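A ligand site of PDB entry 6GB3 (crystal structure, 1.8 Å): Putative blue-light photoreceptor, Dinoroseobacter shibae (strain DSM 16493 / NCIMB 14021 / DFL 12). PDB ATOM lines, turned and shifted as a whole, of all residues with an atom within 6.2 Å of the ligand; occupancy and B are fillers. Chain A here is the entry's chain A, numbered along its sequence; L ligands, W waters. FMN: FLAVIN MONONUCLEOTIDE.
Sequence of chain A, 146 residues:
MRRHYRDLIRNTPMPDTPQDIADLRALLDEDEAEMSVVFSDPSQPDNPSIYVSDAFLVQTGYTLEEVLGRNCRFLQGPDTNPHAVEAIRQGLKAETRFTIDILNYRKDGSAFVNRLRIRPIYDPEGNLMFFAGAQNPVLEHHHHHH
The side-chain amide nitrogen of Gln 135 lies within hydrogen-bond range of an oxygen (O4) of the ligand, at 3.0 Å.
NE2 of Gln 76 sits at hydrogen-bond distance from O4' of the ligand, 2.8 Å away.
The side-chain amide oxygen of Asn 104 is in hydrogen-bond range of a nitrogen (N3) of the ligand (2.8 Å).
The side-chain amide nitrogen of Asn 114 lies within hydrogen-bond range of an oxygen (O4) of the ligand (3.1 Å).
O2P of the ligand lies within salt-bridge range of NH2 of Arg 73 (3.0 Å).
An oxygen (O2') of the ligand sits at hydrogen-bond distance from the backbone NH (N) of Cys 72 (3.4 Å).
OD1 of Asn 71 sits at hydrogen-bond distance from O2' of the ligand, at 2.7 Å.
OD1 of Asn 71 lies within hydrogen-bond range of N of Arg 73.
OD1 of Asn 47 sits at hydrogen-bond distance from OG of Ser 40 (2.7 Å).
OE2 of Glu 86 is in salt-bridge range of NH2 of Arg 89.
The guanidinium group (NH2) of Arg 73 lies within salt-bridge range of the side-chain carboxylate (OD1) of Asp 46 (2.8 Å).
The backbone NH (N) of Asn 114 lies within hydrogen-bond range of the backbone carbonyl oxygen (O) of Ile 102 (2.8 Å).
N of Ser 40 lies within hydrogen-bond range of O of Phe 131 (3.0 Å).
O of Gly 133 sits at hydrogen-bond distance from N of Val 38 (2.8 Å).
The side-chain amide oxygen (OD1) of Asn 104 sits at hydrogen-bond distance from the side-chain amide nitrogen (ND2) of Asn 114 (2.7 Å).
Residues that only touch the ligand: Val 38 (3.7 Å), Ser 40 (3.3 Å), Asn 47 (3.3 Å), Leu 75 (3.2 Å), Val 85 (3.5 Å), Ile 88 (3.6 Å), Arg 89 (3.2 Å), Leu 92 (3.3 Å), Ile 102 (3.7 Å), Leu 116 (3.5 Å), Ile 118 (3.9 Å), Phe 131 (3.8 Å) and Gly 133 (3.6 Å).
Hydrophobic or aromatic side chains within 4 Å of the ligand: Leu 75, Val 85, Ile 88, Leu 92, Ile 102, Leu 116, Ile 118 and Phe 131.
Within 4 Å of the ligand: Val 38, Ser 40, Asn 47, Asn 71, Cys 72, Arg 73, Leu 75, Gln 76, Val 85, Ile 88, Arg 89, Leu 92, Ile 102, Asn 104, Asn 114, Leu 116, Ile 118, Phe 131, Gly 133 and Gln 135.
The nearest printed residue that does not touch the ligand is Ala 132 (4.04 Å).
Water W3 lies within hydrogen-bond range of the backbone carbonyl oxygen (O) of Asn 47 (2.9 Å), the backbone NH (N) of Cys 72 (3.0 Å), an oxygen (O2') of the ligand (3.0 Å) and the side-chain amide nitrogen (ND2) of Asn 71 (3.4 Å).
Water W1 lies within hydrogen-bond range of an oxygen (O3') of the ligand (3.0 Å), the side-chain amide nitrogen of Asn 71 (3.0 Å) and the side-chain amide nitrogen of Asn 47 (3.4 Å).
Water W4 bridges the side-chain carboxylate (OE1) of Glu 86 (2.8 Å) and an oxygen (O1P) of the ligand (3.0 Å).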
ATOM      1  N   VAL A  38      23.607  -4.522  -7.044  1.00  0.00           N
ATOM      2  CA  VAL A  38      24.686  -3.758  -7.650  1.00  0.00           C
ATOM      3  C   VAL A  38      24.054  -2.550  -8.333  1.00  0.00           C
ATOM      4  O   VAL A  38      22.997  -2.671  -8.964  1.00  0.00           O
ATOM      5  CB  VAL A  38      25.452  -4.613  -8.690  1.00  0.00           C
ATOM      6  CG1 VAL A  38      26.451  -3.752  -9.453  1.00  0.00           C
ATOM      7  CG2 VAL A  38      26.164  -5.775  -8.018  1.00  0.00           C
ATOM      8  N   PHE A  39      24.688  -1.386  -8.184  1.00  0.00           N
ATOM      9  CA  PHE A  39      24.382  -0.245  -9.039  1.00  0.00           C
ATOM     10  C   PHE A  39      25.566   0.015  -9.954  1.00  0.00           C
ATOM     11  O   PHE A  39      26.723  -0.030  -9.520  1.00  0.00           O
ATOM     12  CB  PHE A  39      24.075   1.022  -8.239  1.00  0.00           C
ATOM     13  CG  PHE A  39      22.934   0.883  -7.280  1.00  0.00           C
ATOM     14  CD1 PHE A  39      21.662   0.604  -7.736  1.00  0.00           C
ATOM     15  CD2 PHE A  39      23.133   1.046  -5.922  1.00  0.00           C
ATOM     16  CE1 PHE A  39      20.607   0.483  -6.861  1.00  0.00           C
ATOM     17  CE2 PHE A  39      22.073   0.934  -5.037  1.00  0.00           C
ATOM     18  CZ  PHE A  39      20.822   0.656  -5.504  1.00  0.00           C
ATOM     19  N   SER A  40      25.281   0.261 -11.223  1.00  0.00           N
ATOM     20  CA  SER A  40      26.312   0.566 -12.204  1.00  0.00           C
ATOM     21  C   SER A  40      26.101   1.961 -12.762  1.00  0.00           C
ATOM     22  O   SER A  40      25.014   2.530 -12.689  1.00  0.00           O
ATOM     23  CB  SER A  40      26.317  -0.449 -13.348  1.00  0.00           C
ATOM     24  OG  SER A  40      25.237  -0.194 -14.244  1.00  0.00           O
ATOM     25  N   ASP A  46      32.599   1.126 -19.923  1.00  0.00           N
ATOM     26  CA  ASP A  46      32.369  -0.280 -19.604  1.00  0.00           C
ATOM     27  C   ASP A  46      31.382  -0.477 -18.456  1.00  0.00           C
ATOM     28  O   ASP A  46      31.328  -1.550 -17.861  1.00  0.00           O
ATOM     29  CB  ASP A  46      33.693  -0.989 -19.294  1.00  0.00           C
ATOM     30  CG  ASP A  46      33.615  -2.505 -19.447  1.00  0.00           C
ATOM     31  OD1 ASP A  46      32.770  -2.994 -20.231  1.00  0.00           O
ATOM     32  OD2 ASP A  46      34.403  -3.206 -18.764  1.00  0.00           O
ATOM     33  N   ASN A  47      30.579   0.553 -18.136  1.00  0.00           N
ATOM     34  CA  ASN A  47      29.434   0.425 -17.239  1.00  0.00           C
ATOM     35  C   ASN A  47      29.819  -0.230 -15.900  1.00  0.00           C
ATOM     36  O   ASN A  47      29.277  -1.280 -15.538  1.00  0.00           O
ATOM     37  CB  ASN A  47      28.331  -0.355 -17.933  1.00  0.00           C
ATOM     38  CG  ASN A  47      26.986  -0.282 -17.203  1.00  0.00           C
ATOM     39  OD1 ASN A  47      26.750   0.609 -16.387  1.00  0.00           O
ATOM     40  ND2 ASN A  47      26.112  -1.223 -17.508  1.00  0.00           N
ATOM     41  N   PHE A  56      25.886  -9.137  -1.761  1.00  0.00           N
ATOM     42  CA  PHE A  56      26.552  -9.506  -3.010  1.00  0.00           C
ATOM     43  C   PHE A  56      27.942 -10.062  -2.731  1.00  0.00           C
ATOM     44  O   PHE A  56      28.309 -11.137  -3.219  1.00  0.00           O
ATOM     45  CB  PHE A  56      26.649  -8.312  -3.953  1.00  0.00           C
ATOM     46  CG  PHE A  56      27.352  -8.591  -5.263  1.00  0.00           C
ATOM     47  CD1 PHE A  56      28.745  -8.654  -5.342  1.00  0.00           C
ATOM     48  CD2 PHE A  56      26.627  -8.778  -6.417  1.00  0.00           C
ATOM     49  CE1 PHE A  56      29.378  -8.888  -6.535  1.00  0.00           C
ATOM     50  CE2 PHE A  56      27.265  -9.021  -7.621  1.00  0.00           C
ATOM     51  CZ  PHE A  56      28.633  -9.075  -7.679  1.00  0.00           C
ATOM     52  N   ASN A  71      33.093  -3.965 -14.389  1.00  0.00           N
ATOM     53  CA  ASN A  71      31.869  -4.486 -14.989  1.00  0.00           C
ATOM     54  C   ASN A  71      31.545  -5.846 -14.374  1.00  0.00           C
ATOM     55  O   ASN A  71      32.446  -6.658 -14.142  1.00  0.00           O
ATOM     56  CB  ASN A  71      32.041  -4.603 -16.496  1.00  0.00           C
ATOM     57  CG  ASN A  71      30.775  -5.020 -17.200  1.00  0.00           C
ATOM     58  OD1 ASN A  71      30.390  -6.199 -17.161  1.00  0.00           O
ATOM     59  ND2 ASN A  71      30.113  -4.081 -17.850  1.00  0.00           N
ATOM     60  N   CYS A  72      30.261  -6.100 -14.122  1.00  0.00           N
ATOM     61  CA  CYS A  72      29.835  -7.307 -13.401  1.00  0.00           C
ATOM     62  C   CYS A  72      30.033  -8.597 -14.194  1.00  0.00           C
ATOM     63  O   CYS A  72      29.694  -9.664 -13.666  1.00  0.00           O
ATOM     64  CB  CYS A  72      28.370  -7.177 -12.983  1.00  0.00           C
ATOM     65  SG  CYS A  72      28.118  -5.926 -11.728  1.00  0.00           S
ATOM     66  N   ARG A  73      30.583  -8.544 -15.412  1.00  0.00           N
ATOM     67  CA  ARG A  73      30.806  -9.771 -16.168  1.00  0.00           C
ATOM     68  C   ARG A  73      31.810 -10.703 -15.495  1.00  0.00           C
ATOM     69  O   ARG A  73      31.913 -11.860 -15.909  1.00  0.00           O
ATOM     70  CB  ARG A  73      31.283  -9.440 -17.589  1.00  0.00           C
ATOM     71  CG  ARG A  73      32.737  -9.019 -17.663  1.00  0.00           C
ATOM     72  CD  ARG A  73      33.185  -8.864 -19.113  1.00  0.00           C
ATOM     73  NE  ARG A  73      32.406  -7.846 -19.801  1.00  0.00           N
ATOM     74  CZ  ARG A  73      32.686  -6.548 -19.776  1.00  0.00           C
ATOM     75  NH1 ARG A  73      33.739  -6.109 -19.097  1.00  0.00           N
ATOM     76  NH2 ARG A  73      31.911  -5.690 -20.431  1.00  0.00           N
ATOM     77  N   LEU A  75      31.348 -12.136 -12.905  1.00  0.00           N
ATOM     78  CA  LEU A  75      30.527 -13.191 -12.334  1.00  0.00           C
ATOM     79  C   LEU A  75      30.334 -14.366 -13.293  1.00  0.00           C
ATOM     80  O   LEU A  75      29.890 -15.437 -12.864  1.00  0.00           O
ATOM     81  CB  LEU A  75      29.165 -12.625 -11.950  1.00  0.00           C
ATOM     82  CG  LEU A  75      29.260 -11.544 -10.876  1.00  0.00           C
ATOM     83  CD1 LEU A  75      27.957 -10.818 -10.727  1.00  0.00           C
ATOM     84  CD2 LEU A  75      29.679 -12.189  -9.548  1.00  0.00           C
ATOM     85  N   GLN A  76      30.621 -14.178 -14.570  1.00  0.00           N
ATOM     86  CA  GLN A  76      30.431 -15.228 -15.548  1.00  0.00           C
ATOM     87  C   GLN A  76      31.654 -16.122 -15.578  1.00  0.00           C
ATOM     88  O   GLN A  76      32.743 -15.739 -15.165  1.00  0.00           O
ATOM     89  CB  GLN A  76      30.141 -14.608 -16.911  1.00  0.00           C
ATOM     90  CG  GLN A  76      28.871 -13.780 -16.886  1.00  0.00           C
ATOM     91  CD  GLN A  76      28.851 -12.691 -17.926  1.00  0.00           C
ATOM     92  OE1 GLN A  76      29.627 -12.695 -18.879  1.00  0.00           O
ATOM     93  NE2 GLN A  76      27.947 -11.729 -17.748  1.00  0.00           N
ATOM     94  N   THR A  80      28.984 -20.462 -18.559  1.00  0.00           N
ATOM     95  CA  THR A  80      27.943 -19.462 -18.745  1.00  0.00           C
ATOM     96  C   THR A  80      27.527 -19.416 -20.206  1.00  0.00           C
ATOM     97  O   THR A  80      28.368 -19.455 -21.105  1.00  0.00           O
ATOM     98  CB  THR A  80      28.438 -18.091 -18.275  1.00  0.00           C
ATOM     99  OG1 THR A  80      28.792 -18.140 -16.884  1.00  0.00           O
ATOM    100  CG2 THR A  80      27.369 -17.003 -18.483  1.00  0.00           C
ATOM    101  N   VAL A  85      24.382 -13.974 -21.959  1.00  0.00           N
ATOM    102  CA  VAL A  85      25.188 -12.760 -21.830  1.00  0.00           C
ATOM    103  C   VAL A  85      24.771 -11.730 -22.863  1.00  0.00           C
ATOM    104  O   VAL A  85      24.595 -10.539 -22.547  1.00  0.00           O
ATOM    105  CB  VAL A  85      26.685 -13.103 -21.930  1.00  0.00           C
ATOM    106  CG1 VAL A  85      27.524 -11.827 -21.992  1.00  0.00           C
ATOM    107  CG2 VAL A  85      27.100 -13.985 -20.758  1.00  0.00           C
ATOM    108  N   GLU A  86      24.592 -12.150 -24.114  1.00  0.00           N
ATOM    109  CA  GLU A  86      24.170 -11.211 -25.150  1.00  0.00           C
ATOM    110  C   GLU A  86      22.762 -10.677 -24.852  1.00  0.00           C
ATOM    111  O   GLU A  86      22.480  -9.505 -25.106  1.00  0.00           O
ATOM    112  CB  GLU A  86      24.229 -11.884 -26.521  1.00  0.00           C
ATOM    113  CG  GLU A  86      23.911 -10.959 -27.694  1.00  0.00           C
ATOM    114  CD  GLU A  86      24.809  -9.737 -27.770  1.00  0.00           C
ATOM    115  OE1 GLU A  86      25.951  -9.784 -27.260  1.00  0.00           O
ATOM    116  OE2 GLU A  86      24.374  -8.717 -28.348  1.00  0.00           O
ATOM    117  N   ILE A  88      21.438 -10.110 -21.864  1.00  0.00           N
ATOM    118  CA  ILE A  88      21.636  -9.040 -20.891  1.00  0.00           C
ATOM    119  C   ILE A  88      22.136  -7.784 -21.578  1.00  0.00           C
ATOM    120  O   ILE A  88      21.661  -6.672 -21.298  1.00  0.00           O
ATOM    121  CB  ILE A  88      22.600  -9.497 -19.781  1.00  0.00           C
ATOM    122  CG1 ILE A  88      22.042 -10.709 -19.031  1.00  0.00           C
ATOM    123  CG2 ILE A  88      22.920  -8.341 -18.833  1.00  0.00           C
ATOM    124  CD1 ILE A  88      23.055 -11.336 -18.080  1.00  0.00           C
ATOM    125  N   ARG A  89      23.098  -7.933 -22.490  1.00  0.00           N
ATOM    126  CA  ARG A  89      23.663  -6.759 -23.153  1.00  0.00           C
ATOM    127  C   ARG A  89      22.597  -6.012 -23.955  1.00  0.00           C
ATOM    128  O   ARG A  89      22.557  -4.779 -23.931  1.00  0.00           O
ATOM    129  CB  ARG A  89      24.811  -7.177 -24.078  1.00  0.00           C
ATOM    130  CG  ARG A  89      25.759  -6.020 -24.372  1.00  0.00           C
ATOM    131  CD  ARG A  89      26.939  -6.471 -25.192  1.00  0.00           C
ATOM    132  NE  ARG A  89      26.497  -6.791 -26.531  1.00  0.00           N
ATOM    133  CZ  ARG A  89      26.521  -5.935 -27.543  1.00  0.00           C
ATOM    134  NH1 ARG A  89      26.984  -4.712 -27.360  1.00  0.00           N
ATOM    135  NH2 ARG A  89      26.087  -6.301 -28.746  1.00  0.00           N
ATOM    136  N   LEU A  92      20.116  -4.216 -21.577  1.00  0.00           N
ATOM    137  CA  LEU A  92      20.651  -2.952 -21.092  1.00  0.00           C
ATOM    138  C   LEU A  92      20.513  -1.860 -22.154  1.00  0.00           C
ATOM    139  O   LEU A  92      20.132  -0.721 -21.841  1.00  0.00           O
ATOM    140  CB  LEU A  92      22.112  -3.129 -20.692  1.00  0.00           C
ATOM    141  CG  LEU A  92      22.364  -4.052 -19.493  1.00  0.00           C
ATOM    142  CD1 LEU A  92      23.839  -4.314 -19.303  1.00  0.00           C
ATOM    143  CD2 LEU A  92      21.753  -3.464 -18.240  1.00  0.00           C
ATOM    144  N   ILE A 102      20.935 -16.995 -15.261  1.00  0.00           N
ATOM    145  CA  ILE A 102      22.256 -17.139 -15.869  1.00  0.00           C
ATOM    146  C   ILE A 102      23.178 -17.846 -14.882  1.00  0.00           C
ATOM    147  O   ILE A 102      23.108 -17.632 -13.672  1.00  0.00           O
ATOM    148  CB  ILE A 102      22.802 -15.760 -16.299  1.00  0.00           C
ATOM    149  CG1 ILE A 102      24.123 -15.927 -17.057  1.00  0.00           C
ATOM    150  CG2 ILE A 102      22.949 -14.819 -15.093  1.00  0.00           C
ATOM    151  CD1 ILE A 102      24.579 -14.657 -17.749  1.00  0.00           C
ATOM    152  N   LEU A 103      24.043 -18.698 -15.419  1.00  0.00           N
ATOM    153  CA  LEU A 103      25.030 -19.392 -14.593  1.00  0.00           C
ATOM    154  C   LEU A 103      26.129 -18.412 -14.210  1.00  0.00           C
ATOM    155  O   LEU A 103      26.761 -17.815 -15.094  1.00  0.00           O
ATOM    156  CB  LEU A 103      25.597 -20.602 -15.325  1.00  0.00           C
ATOM    157  CG  LEU A 103      26.422 -21.510 -14.419  1.00  0.00           C
ATOM    158  CD1 LEU A 103      25.516 -22.237 -13.425  1.00  0.00           C
ATOM    159  CD2 LEU A 103      27.273 -22.505 -15.230  1.00  0.00           C
ATOM    160  N   ASN A 104      26.346 -18.249 -12.915  1.00  0.00           N
ATOM    161  CA  ASN A 104      27.393 -17.371 -12.397  1.00  0.00           C
ATOM    162  C   ASN A 104      28.317 -18.175 -11.494  1.00  0.00           C
ATOM    163  O   ASN A 104      28.055 -19.329 -11.143  1.00  0.00           O
ATOM    164  CB  ASN A 104      26.796 -16.186 -11.628  1.00  0.00           C
ATOM    165  CG  ASN A 104      26.290 -15.069 -12.541  1.00  0.00           C
ATOM    166  OD1 ASN A 104      25.685 -14.115 -12.065  1.00  0.00           O
ATOM    167  ND2 ASN A 104      26.533 -15.197 -13.851  1.00  0.00           N
ATOM    168  N   ASN A 114      21.894 -17.865 -11.161  1.00  0.00           N
ATOM    169  CA  ASN A 114      21.573 -16.525 -10.695  1.00  0.00           C
ATOM    170  C   ASN A 114      20.346 -16.020 -11.443  1.00  0.00           C
ATOM    171  O   ASN A 114      20.379 -15.890 -12.673  1.00  0.00           O
ATOM    172  CB  ASN A 114      22.771 -15.590 -10.901  1.00  0.00           C
ATOM    173  CG  ASN A 114      22.463 -14.149 -10.549  1.00  0.00           C
ATOM    174  OD1 ASN A 114      21.442 -13.851  -9.919  1.00  0.00           O
ATOM    175  ND2 ASN A 114      23.357 -13.244 -10.950  1.00  0.00           N
ATOM    176  N   LEU A 116      18.846 -12.941 -12.243  1.00  0.00           N
ATOM    177  CA  LEU A 116      19.319 -11.567 -12.281  1.00  0.00           C
ATOM    178  C   LEU A 116      18.188 -10.663 -12.740  1.00  0.00           C
ATOM    179  O   LEU A 116      17.620 -10.889 -13.812  1.00  0.00           O
ATOM    180  CB  LEU A 116      20.497 -11.453 -13.230  1.00  0.00           C
ATOM    181  CG  LEU A 116      20.987 -10.039 -13.548  1.00  0.00           C
ATOM    182  CD1 LEU A 116      21.528  -9.390 -12.271  1.00  0.00           C
ATOM    183  CD2 LEU A 116      22.060 -10.128 -14.621  1.00  0.00           C
ATOM    184  N   ILE A 118      17.333  -6.678 -13.612  1.00  0.00           N
ATOM    185  CA  ILE A 118      17.964  -5.392 -13.907  1.00  0.00           C
ATOM    186  C   ILE A 118      16.887  -4.381 -14.252  1.00  0.00           C
ATOM    187  O   ILE A 118      15.909  -4.714 -14.938  1.00  0.00           O
ATOM    188  CB  ILE A 118      19.011  -5.521 -15.027  1.00  0.00           C
ATOM    189  CG1 ILE A 118      20.253  -6.235 -14.491  1.00  0.00           C
ATOM    190  CG2 ILE A 118      19.387  -4.165 -15.593  1.00  0.00           C
ATOM    191  CD1 ILE A 118      21.282  -6.569 -15.539  1.00  0.00           C
ATOM    192  N   PHE A 131      22.051   1.771 -13.641  1.00  0.00           N
ATOM    193  CA  PHE A 131      21.333   0.500 -13.665  1.00  0.00           C
ATOM    194  C   PHE A 131      21.359  -0.084 -12.264  1.00  0.00           C
ATOM    195  O   PHE A 131      22.350   0.065 -11.529  1.00  0.00           O
ATOM    196  CB  PHE A 131      21.965  -0.484 -14.655  1.00  0.00           C
ATOM    197  CG  PHE A 131      21.680  -0.176 -16.102  1.00  0.00           C
ATOM    198  CD1 PHE A 131      20.423  -0.397 -16.652  1.00  0.00           C
ATOM    199  CD2 PHE A 131      22.690   0.297 -16.930  1.00  0.00           C
ATOM    200  CE1 PHE A 131      20.156  -0.120 -17.991  1.00  0.00           C
ATOM    201  CE2 PHE A 131      22.435   0.564 -18.273  1.00  0.00           C
ATOM    202  CZ  PHE A 131      21.169   0.360 -18.803  1.00  0.00           C
ATOM    203  N   ALA A 132      20.267  -0.736 -11.874  1.00  0.00           N
ATOM    204  CA  ALA A 132      20.194  -1.506 -10.639  1.00  0.00           C
ATOM    205  C   ALA A 132      20.057  -2.976 -11.015  1.00  0.00           C
ATOM    206  O   ALA A 132      19.194  -3.327 -11.819  1.00  0.00           O
ATOM    207  CB  ALA A 132      19.042  -1.072  -9.740  1.00  0.00           C
ATOM    208  N   GLY A 133      20.898  -3.816 -10.434  1.00  0.00           N
ATOM    209  CA  GLY A 133      20.856  -5.233 -10.699  1.00  0.00           C
ATOM    210  C   GLY A 133      20.794  -6.004  -9.407  1.00  0.00           C
ATOM    211  O   GLY A 133      21.629  -5.809  -8.519  1.00  0.00           O
ATOM    212  N   ALA A 134      19.790  -6.863  -9.264  1.00  0.00           N
ATOM    213  CA  ALA A 134      19.602  -7.622  -8.036  1.00  0.00           C
ATOM    214  C   ALA A 134      19.798  -9.100  -8.361  1.00  0.00           C
ATOM    215  O   ALA A 134      19.258  -9.596  -9.360  1.00  0.00           O
ATOM    216  CB  ALA A 134      18.221  -7.371  -7.433  1.00  0.00           C
ATOM    217  N   GLN A 135      20.576  -9.786  -7.534  1.00  0.00           N
ATOM    218  CA  GLN A 135      20.891 -11.192  -7.742  1.00  0.00           C
ATOM    219  C   GLN A 135      20.154 -12.049  -6.731  1.00  0.00           C
ATOM    220  O   GLN A 135      20.109 -11.744  -5.530  1.00  0.00           O
ATOM    221  CB  GLN A 135      22.395 -11.452  -7.630  1.00  0.00           C
ATOM    222  CG  GLN A 135      23.234 -10.767  -8.700  1.00  0.00           C
ATOM    223  CD  GLN A 135      23.524  -9.318  -8.391  1.00  0.00           C
ATOM    224  OE1 GLN A 135      23.337  -8.856  -7.259  1.00  0.00           O
ATOM    225  NE2 GLN A 135      23.996  -8.583  -9.396  1.00  0.00           N
HETATM  226  N1  FMN L   1      25.967 -10.343 -15.311  1.00  0.00           N
HETATM  227  C2  FMN L   1      26.012 -11.549 -14.650  1.00  0.00           C
HETATM  228  O2  FMN L   1      26.378 -12.554 -15.240  1.00  0.00           O
HETATM  229  N3  FMN L   1      25.640 -11.627 -13.322  1.00  0.00           N
HETATM  230  C4  FMN L   1      25.218 -10.513 -12.634  1.00  0.00           C
HETATM  231  O4  FMN L   1      24.891 -10.610 -11.449  1.00  0.00           O
HETATM  232  C4A FMN L   1      25.181  -9.287 -13.300  1.00  0.00           C
HETATM  233  N5  FMN L   1      24.778  -8.160 -12.635  1.00  0.00           N
HETATM  234  C5A FMN L   1      24.722  -6.950 -13.315  1.00  0.00           C
HETATM  235  C6  FMN L   1      24.300  -5.814 -12.638  1.00  0.00           C
HETATM  236  C7  FMN L   1      24.237  -4.589 -13.285  1.00  0.00           C
HETATM  237  C7M FMN L   1      23.784  -3.374 -12.521  1.00  0.00           C
HETATM  238  C8  FMN L   1      24.607  -4.508 -14.627  1.00  0.00           C
HETATM  239  C8M FMN L   1      24.551  -3.179 -15.342  1.00  0.00           C
HETATM  240  C9  FMN L   1      25.035  -5.643 -15.312  1.00  0.00           C
HETATM  241  C9A FMN L   1      25.092  -6.869 -14.657  1.00  0.00           C
HETATM  242  N10 FMN L   1      25.533  -8.012 -15.310  1.00  0.00           N
HETATM  243  C10 FMN L   1      25.559  -9.208 -14.636  1.00  0.00           C
HETATM  244  C1' FMN L   1      25.906  -8.011 -16.771  1.00  0.00           C
HETATM  245  C2' FMN L   1      27.345  -7.657 -17.147  1.00  0.00           C
HETATM  246  O2' FMN L   1      27.772  -6.517 -16.434  1.00  0.00           O
HETATM  247  C3' FMN L   1      27.363  -7.325 -18.635  1.00  0.00           C
HETATM  248  O3' FMN L   1      26.414  -6.303 -18.876  1.00  0.00           O
HETATM  249  C4' FMN L   1      27.028  -8.549 -19.491  1.00  0.00           C
HETATM  250  O4' FMN L   1      28.091  -9.471 -19.403  1.00  0.00           O
HETATM  251  C5' FMN L   1      26.791  -8.199 -20.960  1.00  0.00           C
HETATM  252  O5' FMN L   1      27.769  -7.266 -21.384  1.00  0.00           O
HETATM  253  P   FMN L   1      29.086  -7.791 -22.139  1.00  0.00           P
HETATM  254  O1P FMN L   1      28.626  -8.535 -23.383  1.00  0.00           O
HETATM  255  O2P FMN L   1      29.944  -6.593 -22.505  1.00  0.00           O
HETATM  256  O3P FMN L   1      29.868  -8.717 -21.229  1.00  0.00           O
HETATM  257  O   HOH W   1      27.580  -3.621 -19.470  1.00  0.00           O
HETATM  258  O   HOH W   2      28.662  -4.152 -22.489  1.00  0.00           O
HETATM  259  O   HOH W   3      28.367  -4.006 -14.989  1.00  0.00           O
HETATM  260  O   HOH W   4      27.827 -10.621 -25.389  1.00  0.00           O
